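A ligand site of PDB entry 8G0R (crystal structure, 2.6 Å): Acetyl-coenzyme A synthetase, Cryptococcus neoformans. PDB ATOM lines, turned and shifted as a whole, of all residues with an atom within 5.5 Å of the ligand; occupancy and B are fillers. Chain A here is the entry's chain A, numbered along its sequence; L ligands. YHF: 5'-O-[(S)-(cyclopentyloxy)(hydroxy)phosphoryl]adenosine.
O3 of the ligand is in hydrogen-bond range of OD1 of Asp 541 (2.5 Å). An oxygen (O1) of the ligand lies within hydrogen-bond range of the guanidinium group (NH1) of Arg 556. N of Thr 455 is in hydrogen-bond range of O6 of the ligand (3.0 Å). The side-chain hydroxyl (OG1) of Thr 455 lies within hydrogen-bond range of an oxygen (O5) of the ligand. N5 of the ligand sits at hydrogen-bond distance from O of Thr 451. The side-chain carboxylate (OD1) of Asp 450 sits at hydrogen-bond distance from a nitrogen (N5) of the ligand (3.1 Å). A nitrogen (N2) of the ligand lies within hydrogen-bond range of the backbone NH (N) of Gly 426 (3.3 Å). An oxygen (O1) of the ligand sits at hydrogen-bond distance from the side-chain sulfur (SD) of Met 454 (3.1 Å).
The guanidinium group (NH1) of Arg 556 lies within salt-bridge range of the side-chain carboxylate (OD1) of Asp 541, at 3.7 Å. The side-chain carboxylate of Asp 541 sits at hydrogen-bond distance from the side-chain hydroxyl of Tyr 452. The guanidinium group (NH1) of Arg 556 lies within hydrogen-bond range of the backbone carbonyl oxygen (O) of Phe 539, 3.4 Å away. The side-chain hydroxyl (OG1) of Thr 451 lies within hydrogen-bond range of the backbone carbonyl oxygen (O) of Ser 424.
N of Pro 428 lies close to N3 of the ligand, 3.5 Å away. Merely in contact with the ligand: Ile 349 (3.4 Å), Thr 350 (3.3 Å), Val 425 (3.3 Å), Glu 427 (3.5 Å), Tyr 452 (3.5 Å), Trp 453 (3.4 Å), Glu 456 (3.99 Å) and Ile 553 (3.5 Å). Hydrophobic or aromatic side chains that line the ligand: Ile 349, Val 425, Pro 428, Tyr 452, Trp 453, Met 454 and Ile 553. Along chain A the residues within 4 Å of the ligand span positions 349 to 556. The nearest printed residue that does not touch the ligand is Ser 424 (4.5 Å).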
ATOM      1  N   THR A 303     -14.130 -26.587 -22.139  1.00  0.00           N
ATOM      2  CA  THR A 303     -14.243 -25.585 -21.087  1.00  0.00           C
ATOM      3  C   THR A 303     -15.708 -25.216 -20.896  1.00  0.00           C
ATOM      4  O   THR A 303     -16.497 -25.219 -21.845  1.00  0.00           O
ATOM      5  CB  THR A 303     -13.438 -24.336 -21.416  1.00  0.00           C
ATOM      6  OG1 THR A 303     -13.961 -23.717 -22.604  1.00  0.00           O
ATOM      7  CG2 THR A 303     -11.968 -24.678 -21.631  1.00  0.00           C
ATOM      8  N   ILE A 349      -7.409 -28.673 -16.736  1.00  0.00           N
ATOM      9  CA  ILE A 349      -6.085 -28.628 -17.364  1.00  0.00           C
ATOM     10  C   ILE A 349      -5.005 -28.776 -16.307  1.00  0.00           C
ATOM     11  O   ILE A 349      -3.899 -29.251 -16.597  1.00  0.00           O
ATOM     12  CB  ILE A 349      -5.925 -27.339 -18.175  1.00  0.00           C
ATOM     13  CG1 ILE A 349      -4.620 -27.388 -18.982  1.00  0.00           C
ATOM     14  CG2 ILE A 349      -5.929 -26.140 -17.260  1.00  0.00           C
ATOM     15  CD1 ILE A 349      -4.653 -28.399 -20.099  1.00  0.00           C
ATOM     16  N   THR A 350      -5.291 -28.357 -15.074  1.00  0.00           N
ATOM     17  CA  THR A 350      -4.294 -28.466 -14.012  1.00  0.00           C
ATOM     18  C   THR A 350      -3.940 -29.920 -13.751  1.00  0.00           C
ATOM     19  O   THR A 350      -2.767 -30.240 -13.491  1.00  0.00           O
ATOM     20  CB  THR A 350      -4.837 -27.804 -12.737  1.00  0.00           C
ATOM     21  OG1 THR A 350      -5.296 -26.486 -13.045  1.00  0.00           O
ATOM     22  CG2 THR A 350      -3.743 -27.715 -11.681  1.00  0.00           C
ATOM     23  N   SER A 424      -0.233 -22.036  -6.205  1.00  0.00           N
ATOM     24  CA  SER A 424      -1.620 -21.592  -6.265  1.00  0.00           C
ATOM     25  C   SER A 424      -1.998 -21.364  -7.724  1.00  0.00           C
ATOM     26  O   SER A 424      -1.209 -20.832  -8.506  1.00  0.00           O
ATOM     27  CB  SER A 424      -1.835 -20.312  -5.458  1.00  0.00           C
ATOM     28  OG  SER A 424      -3.177 -19.881  -5.552  1.00  0.00           O
ATOM     29  N   VAL A 425      -3.221 -21.742  -8.078  1.00  0.00           N
ATOM     30  CA  VAL A 425      -3.661 -21.708  -9.467  1.00  0.00           C
ATOM     31  C   VAL A 425      -5.171 -21.572  -9.515  1.00  0.00           C
ATOM     32  O   VAL A 425      -5.895 -22.007  -8.621  1.00  0.00           O
ATOM     33  CB  VAL A 425      -3.201 -22.981 -10.210  1.00  0.00           C
ATOM     34  CG1 VAL A 425      -3.663 -24.231  -9.467  1.00  0.00           C
ATOM     35  CG2 VAL A 425      -3.731 -22.989 -11.632  1.00  0.00           C
ATOM     36  N   GLY A 426      -5.652 -20.935 -10.589  1.00  0.00           N
ATOM     37  CA  GLY A 426      -7.069 -20.863 -10.881  1.00  0.00           C
ATOM     38  C   GLY A 426      -7.618 -19.451 -10.960  1.00  0.00           C
ATOM     39  O   GLY A 426      -8.400 -19.164 -11.869  1.00  0.00           O
ATOM     40  N   GLU A 427      -7.207 -18.575 -10.056  1.00  0.00           N
ATOM     41  CA  GLU A 427      -7.708 -17.200 -10.000  1.00  0.00           C
ATOM     42  C   GLU A 427      -6.755 -16.406  -9.117  1.00  0.00           C
ATOM     43  O   GLU A 427      -5.935 -16.989  -8.385  1.00  0.00           O
ATOM     44  CB  GLU A 427      -9.143 -17.170  -9.438  1.00  0.00           C
ATOM     45  CG  GLU A 427     -10.204 -17.640 -10.422  1.00  0.00           C
ATOM     46  CD  GLU A 427     -11.616 -17.306  -9.994  1.00  0.00           C
ATOM     47  OE1 GLU A 427     -11.799 -16.609  -8.975  1.00  0.00           O
ATOM     48  OE2 GLU A 427     -12.562 -17.725 -10.700  1.00  0.00           O
ATOM     49  N   PRO A 428      -6.855 -15.079  -9.134  1.00  0.00           N
ATOM     50  CA  PRO A 428      -6.003 -14.282  -8.232  1.00  0.00           C
ATOM     51  C   PRO A 428      -6.148 -14.726  -6.776  1.00  0.00           C
ATOM     52  O   PRO A 428      -7.275 -14.877  -6.272  1.00  0.00           O
ATOM     53  CB  PRO A 428      -6.484 -12.840  -8.432  1.00  0.00           C
ATOM     54  CG  PRO A 428      -7.157 -12.838  -9.768  1.00  0.00           C
ATOM     55  CD  PRO A 428      -7.752 -14.217  -9.935  1.00  0.00           C
ATOM     56  N   ILE A 429      -5.019 -14.949  -6.109  1.00  0.00           N
ATOM     57  CA  ILE A 429      -5.012 -15.257  -4.683  1.00  0.00           C
ATOM     58  C   ILE A 429      -4.892 -13.956  -3.906  1.00  0.00           C
ATOM     59  O   ILE A 429      -3.887 -13.253  -4.013  1.00  0.00           O
ATOM     60  CB  ILE A 429      -3.870 -16.225  -4.328  1.00  0.00           C
ATOM     61  CG1 ILE A 429      -3.964 -16.647  -2.861  1.00  0.00           C
ATOM     62  CG2 ILE A 429      -2.510 -15.583  -4.591  1.00  0.00           C
ATOM     63  CD1 ILE A 429      -2.934 -17.666  -2.436  1.00  0.00           C
ATOM     64  N   ASP A 450       2.713 -18.385  -7.364  1.00  0.00           N
ATOM     65  CA  ASP A 450       1.389 -18.044  -7.890  1.00  0.00           C
ATOM     66  C   ASP A 450       1.445 -18.241  -9.401  1.00  0.00           C
ATOM     67  O   ASP A 450       1.978 -17.409 -10.131  1.00  0.00           O
ATOM     68  CB  ASP A 450       1.017 -16.618  -7.513  1.00  0.00           C
ATOM     69  CG  ASP A 450      -0.408 -16.265  -7.888  1.00  0.00           C
ATOM     70  OD1 ASP A 450      -1.188 -17.201  -8.175  1.00  0.00           O
ATOM     71  OD2 ASP A 450      -0.739 -15.066  -7.905  1.00  0.00           O
ATOM     72  N   THR A 451       0.867 -19.348  -9.871  1.00  0.00           N
ATOM     73  CA  THR A 451       1.005 -19.764 -11.253  1.00  0.00           C
ATOM     74  C   THR A 451      -0.211 -19.310 -12.053  1.00  0.00           C
ATOM     75  O   THR A 451      -1.314 -19.824 -11.868  1.00  0.00           O
ATOM     76  CB  THR A 451       1.163 -21.287 -11.347  1.00  0.00           C
ATOM     77  OG1 THR A 451      -0.026 -21.920 -10.853  1.00  0.00           O
ATOM     78  CG2 THR A 451       2.361 -21.755 -10.546  1.00  0.00           C
ATOM     79  N   TYR A 452       0.015 -18.338 -12.943  1.00  0.00           N
ATOM     80  CA  TYR A 452      -1.030 -17.865 -13.851  1.00  0.00           C
ATOM     81  C   TYR A 452      -0.916 -18.595 -15.178  1.00  0.00           C
ATOM     82  O   TYR A 452       0.177 -18.682 -15.754  1.00  0.00           O
ATOM     83  CB  TYR A 452      -0.919 -16.363 -14.073  1.00  0.00           C
ATOM     84  CG  TYR A 452      -1.747 -15.880 -15.237  1.00  0.00           C
ATOM     85  CD1 TYR A 452      -3.103 -15.609 -15.089  1.00  0.00           C
ATOM     86  CD2 TYR A 452      -1.190 -15.706 -16.499  1.00  0.00           C
ATOM     87  CE1 TYR A 452      -3.871 -15.172 -16.146  1.00  0.00           C
ATOM     88  CE2 TYR A 452      -1.948 -15.274 -17.565  1.00  0.00           C
ATOM     89  CZ  TYR A 452      -3.289 -15.006 -17.383  1.00  0.00           C
ATOM     90  OH  TYR A 452      -4.047 -14.574 -18.449  1.00  0.00           O
ATOM     91  N   TRP A 453      -2.029 -19.108 -15.669  1.00  0.00           N
ATOM     92  CA  TRP A 453      -2.115 -19.692 -17.001  1.00  0.00           C
ATOM     93  C   TRP A 453      -3.583 -20.035 -17.263  1.00  0.00           C
ATOM     94  O   TRP A 453      -4.452 -19.824 -16.410  1.00  0.00           O
ATOM     95  CB  TRP A 453      -1.200 -20.914 -17.154  1.00  0.00           C
ATOM     96  CG  TRP A 453      -1.443 -22.043 -16.177  1.00  0.00           C
ATOM     97  CD1 TRP A 453      -1.352 -21.976 -14.811  1.00  0.00           C
ATOM     98  CD2 TRP A 453      -1.752 -23.405 -16.481  1.00  0.00           C
ATOM     99  NE1 TRP A 453      -1.614 -23.199 -14.257  1.00  0.00           N
ATOM    100  CE2 TRP A 453      -1.861 -24.097 -15.263  1.00  0.00           C
ATOM    101  CE3 TRP A 453      -1.956 -24.105 -17.682  1.00  0.00           C
ATOM    102  CZ2 TRP A 453      -2.159 -25.458 -15.199  1.00  0.00           C
ATOM    103  CZ3 TRP A 453      -2.264 -25.461 -17.610  1.00  0.00           C
ATOM    104  CH2 TRP A 453      -2.355 -26.126 -16.374  1.00  0.00           C
ATOM    105  N   MET A 454      -3.844 -20.553 -18.452  1.00  0.00           N
ATOM    106  CA  MET A 454      -5.193 -20.917 -18.872  1.00  0.00           C
ATOM    107  C   MET A 454      -5.150 -22.296 -19.515  1.00  0.00           C
ATOM    108  O   MET A 454      -4.095 -22.811 -19.865  1.00  0.00           O
ATOM    109  CB  MET A 454      -5.770 -19.904 -19.862  1.00  0.00           C
ATOM    110  CG  MET A 454      -5.460 -18.471 -19.519  1.00  0.00           C
ATOM    111  SD  MET A 454      -6.236 -17.324 -20.676  1.00  0.00           S
ATOM    112  CE  MET A 454      -5.680 -17.999 -22.243  1.00  0.00           C
ATOM    113  N   THR A 455      -6.334 -22.868 -19.696  1.00  0.00           N
ATOM    114  CA  THR A 455      -6.423 -24.113 -20.449  1.00  0.00           C
ATOM    115  C   THR A 455      -5.804 -23.973 -21.831  1.00  0.00           C
ATOM    116  O   THR A 455      -5.200 -24.914 -22.343  1.00  0.00           O
ATOM    117  CB  THR A 455      -7.890 -24.548 -20.571  1.00  0.00           C
ATOM    118  OG1 THR A 455      -8.443 -24.695 -19.263  1.00  0.00           O
ATOM    119  CG2 THR A 455      -7.993 -25.856 -21.335  1.00  0.00           C
ATOM    120  N   GLU A 456      -5.922 -22.786 -22.448  1.00  0.00           N
ATOM    121  CA  GLU A 456      -5.434 -22.582 -23.804  1.00  0.00           C
ATOM    122  C   GLU A 456      -3.929 -22.368 -23.872  1.00  0.00           C
ATOM    123  O   GLU A 456      -3.345 -22.492 -24.954  1.00  0.00           O
ATOM    124  CB  GLU A 456      -6.127 -21.381 -24.441  1.00  0.00           C
ATOM    125  CG  GLU A 456      -7.636 -21.532 -24.569  1.00  0.00           C
ATOM    126  CD  GLU A 456      -8.380 -21.049 -23.334  1.00  0.00           C
ATOM    127  OE1 GLU A 456      -7.807 -21.071 -22.229  1.00  0.00           O
ATOM    128  OE2 GLU A 456      -9.559 -20.646 -23.488  1.00  0.00           O
ATOM    129  N   ALA A 476       1.823 -12.993  -9.828  1.00  0.00           N
ATOM    130  CA  ALA A 476       2.424 -14.060 -10.624  1.00  0.00           C
ATOM    131  C   ALA A 476       3.867 -13.758 -10.991  1.00  0.00           C
ATOM    132  O   ALA A 476       4.555 -14.639 -11.515  1.00  0.00           O
ATOM    133  CB  ALA A 476       1.610 -14.283 -11.893  1.00  0.00           C
ATOM    134  N   PHE A 539      -5.291 -13.306 -23.866  1.00  0.00           N
ATOM    135  CA  PHE A 539      -5.692 -14.195 -22.785  1.00  0.00           C
ATOM    136  C   PHE A 539      -7.139 -13.946 -22.366  1.00  0.00           C
ATOM    137  O   PHE A 539      -7.884 -14.899 -22.095  1.00  0.00           O
ATOM    138  CB  PHE A 539      -4.771 -14.005 -21.570  1.00  0.00           C
ATOM    139  CG  PHE A 539      -3.354 -14.446 -21.793  1.00  0.00           C
ATOM    140  CD1 PHE A 539      -2.976 -15.761 -21.576  1.00  0.00           C
ATOM    141  CD2 PHE A 539      -2.383 -13.535 -22.187  1.00  0.00           C
ATOM    142  CE1 PHE A 539      -1.667 -16.160 -21.767  1.00  0.00           C
ATOM    143  CE2 PHE A 539      -1.075 -13.933 -22.378  1.00  0.00           C
ATOM    144  CZ  PHE A 539      -0.718 -15.251 -22.173  1.00  0.00           C
ATOM    145  N   ASP A 541      -7.600 -11.435 -19.836  1.00  0.00           N
ATOM    146  CA  ASP A 541      -7.416 -10.947 -18.476  1.00  0.00           C
ATOM    147  C   ASP A 541      -6.887  -9.519 -18.498  1.00  0.00           C
ATOM    148  O   ASP A 541      -6.098  -9.154 -19.372  1.00  0.00           O
ATOM    149  CB  ASP A 541      -6.422 -11.822 -17.693  1.00  0.00           C
ATOM    150  CG  ASP A 541      -6.988 -13.164 -17.323  1.00  0.00           C
ATOM    151  OD1 ASP A 541      -8.147 -13.230 -16.868  1.00  0.00           O
ATOM    152  OD2 ASP A 541      -6.248 -14.172 -17.462  1.00  0.00           O
ATOM    153  N   ILE A 553      -2.144 -10.076 -12.198  1.00  0.00           N
ATOM    154  CA  ILE A 553      -3.352 -10.486 -12.901  1.00  0.00           C
ATOM    155  C   ILE A 553      -4.546 -10.124 -12.027  1.00  0.00           C
ATOM    156  O   ILE A 553      -4.720 -10.661 -10.936  1.00  0.00           O
ATOM    157  CB  ILE A 553      -3.328 -11.999 -13.205  1.00  0.00           C
ATOM    158  CG1 ILE A 553      -1.988 -12.384 -13.845  1.00  0.00           C
ATOM    159  CG2 ILE A 553      -4.487 -12.360 -14.117  1.00  0.00           C
ATOM    160  CD1 ILE A 553      -1.641 -11.615 -15.094  1.00  0.00           C
ATOM    161  N   GLY A 555      -7.938 -10.115 -12.950  1.00  0.00           N
ATOM    162  CA  GLY A 555      -9.200 -10.748 -13.271  1.00  0.00           C
ATOM    163  C   GLY A 555      -9.582 -10.606 -14.725  1.00  0.00           C
ATOM    164  O   GLY A 555      -8.926  -9.926 -15.517  1.00  0.00           O
ATOM    165  N   ARG A 556     -10.671 -11.288 -15.081  1.00  0.00           N
ATOM    166  CA  ARG A 556     -11.132 -11.320 -16.450  1.00  0.00           C
ATOM    167  C   ARG A 556     -11.461  -9.911 -16.956  1.00  0.00           C
ATOM    168  O   ARG A 556     -11.886  -9.040 -16.198  1.00  0.00           O
ATOM    169  CB  ARG A 556     -12.378 -12.201 -16.592  1.00  0.00           C
ATOM    170  CG  ARG A 556     -12.179 -13.655 -16.204  1.00  0.00           C
ATOM    171  CD  ARG A 556     -11.214 -14.396 -17.134  1.00  0.00           C
ATOM    172  NE  ARG A 556     -11.652 -14.387 -18.530  1.00  0.00           N
ATOM    173  CZ  ARG A 556     -10.954 -14.907 -19.538  1.00  0.00           C
ATOM    174  NH1 ARG A 556      -9.796 -15.514 -19.329  1.00  0.00           N
ATOM    175  NH2 ARG A 556     -11.430 -14.813 -20.769  1.00  0.00           N
ATOM    176  N   SER A 652     -14.513 -26.539 -11.071  1.00  0.00           N
ATOM    177  CA  SER A 652     -13.099 -26.239 -10.981  1.00  0.00           C
ATOM    178  C   SER A 652     -12.795 -25.261  -9.851  1.00  0.00           C
ATOM    179  O   SER A 652     -11.655 -25.205  -9.376  1.00  0.00           O
ATOM    180  CB  SER A 652     -12.600 -25.660 -12.302  1.00  0.00           C
ATOM    181  OG  SER A 652     -13.405 -24.577 -12.725  1.00  0.00           O
HETATM  182  C1  YHF L   1      -7.284 -17.165 -16.645  1.00  0.00           C
HETATM  183  C10 YHF L   1      -8.107 -19.588 -16.870  1.00  0.00           C
HETATM  184  C11 YHF L   1      -7.193 -23.065 -16.030  1.00  0.00           C
HETATM  185  C12 YHF L   1      -5.653 -23.070 -15.891  1.00  0.00           C
HETATM  186  C13 YHF L   1      -5.354 -23.485 -14.446  1.00  0.00           C
HETATM  187  C14 YHF L   1      -6.651 -23.451 -13.717  1.00  0.00           C
HETATM  188  C15 YHF L   1      -7.544 -22.591 -14.610  1.00  0.00           C
HETATM  189  C2  YHF L   1      -7.494 -16.154 -15.522  1.00  0.00           C
HETATM  190  C3  YHF L   1      -7.690 -17.052 -14.316  1.00  0.00           C
HETATM  191  C4  YHF L   1      -5.808 -18.650 -13.515  1.00  0.00           C
HETATM  192  C5  YHF L   1      -4.661 -17.350 -12.255  1.00  0.00           C
HETATM  193  C6  YHF L   1      -5.712 -16.586 -12.747  1.00  0.00           C
HETATM  194  C7  YHF L   1      -5.049 -14.793 -11.667  1.00  0.00           C
HETATM  195  C8  YHF L   1      -3.758 -16.701 -11.381  1.00  0.00           C
HETATM  196  C9  YHF L   1      -8.314 -18.236 -16.239  1.00  0.00           C
HETATM  197  N1  YHF L   1      -6.453 -17.422 -13.560  1.00  0.00           N
HETATM  198  N2  YHF L   1      -4.728 -18.637 -12.742  1.00  0.00           N
HETATM  199  N3  YHF L   1      -5.966 -15.296 -12.487  1.00  0.00           N
HETATM  200  N4  YHF L   1      -3.992 -15.386 -11.113  1.00  0.00           N
HETATM  201  N5  YHF L   1      -2.699 -17.296 -10.837  1.00  0.00           N
HETATM  202  O1  YHF L   1      -7.569 -16.681 -17.947  1.00  0.00           O
HETATM  203  O2  YHF L   1      -8.191 -18.296 -14.805  1.00  0.00           O
HETATM  204  O3  YHF L   1      -8.680 -15.397 -15.711  1.00  0.00           O
HETATM  205  O4  YHF L   1      -9.183 -20.462 -16.474  1.00  0.00           O
HETATM  206  O5  YHF L   1      -9.483 -21.674 -18.664  1.00  0.00           O
HETATM  207  O6  YHF L   1      -7.613 -22.216 -17.055  1.00  0.00           O
HETATM  208  O7  YHF L   1     -10.026 -22.818 -16.427  1.00  0.00           O
HETATM  209  P1  YHF L   1      -9.174 -21.884 -17.215  1.00  0.00           P
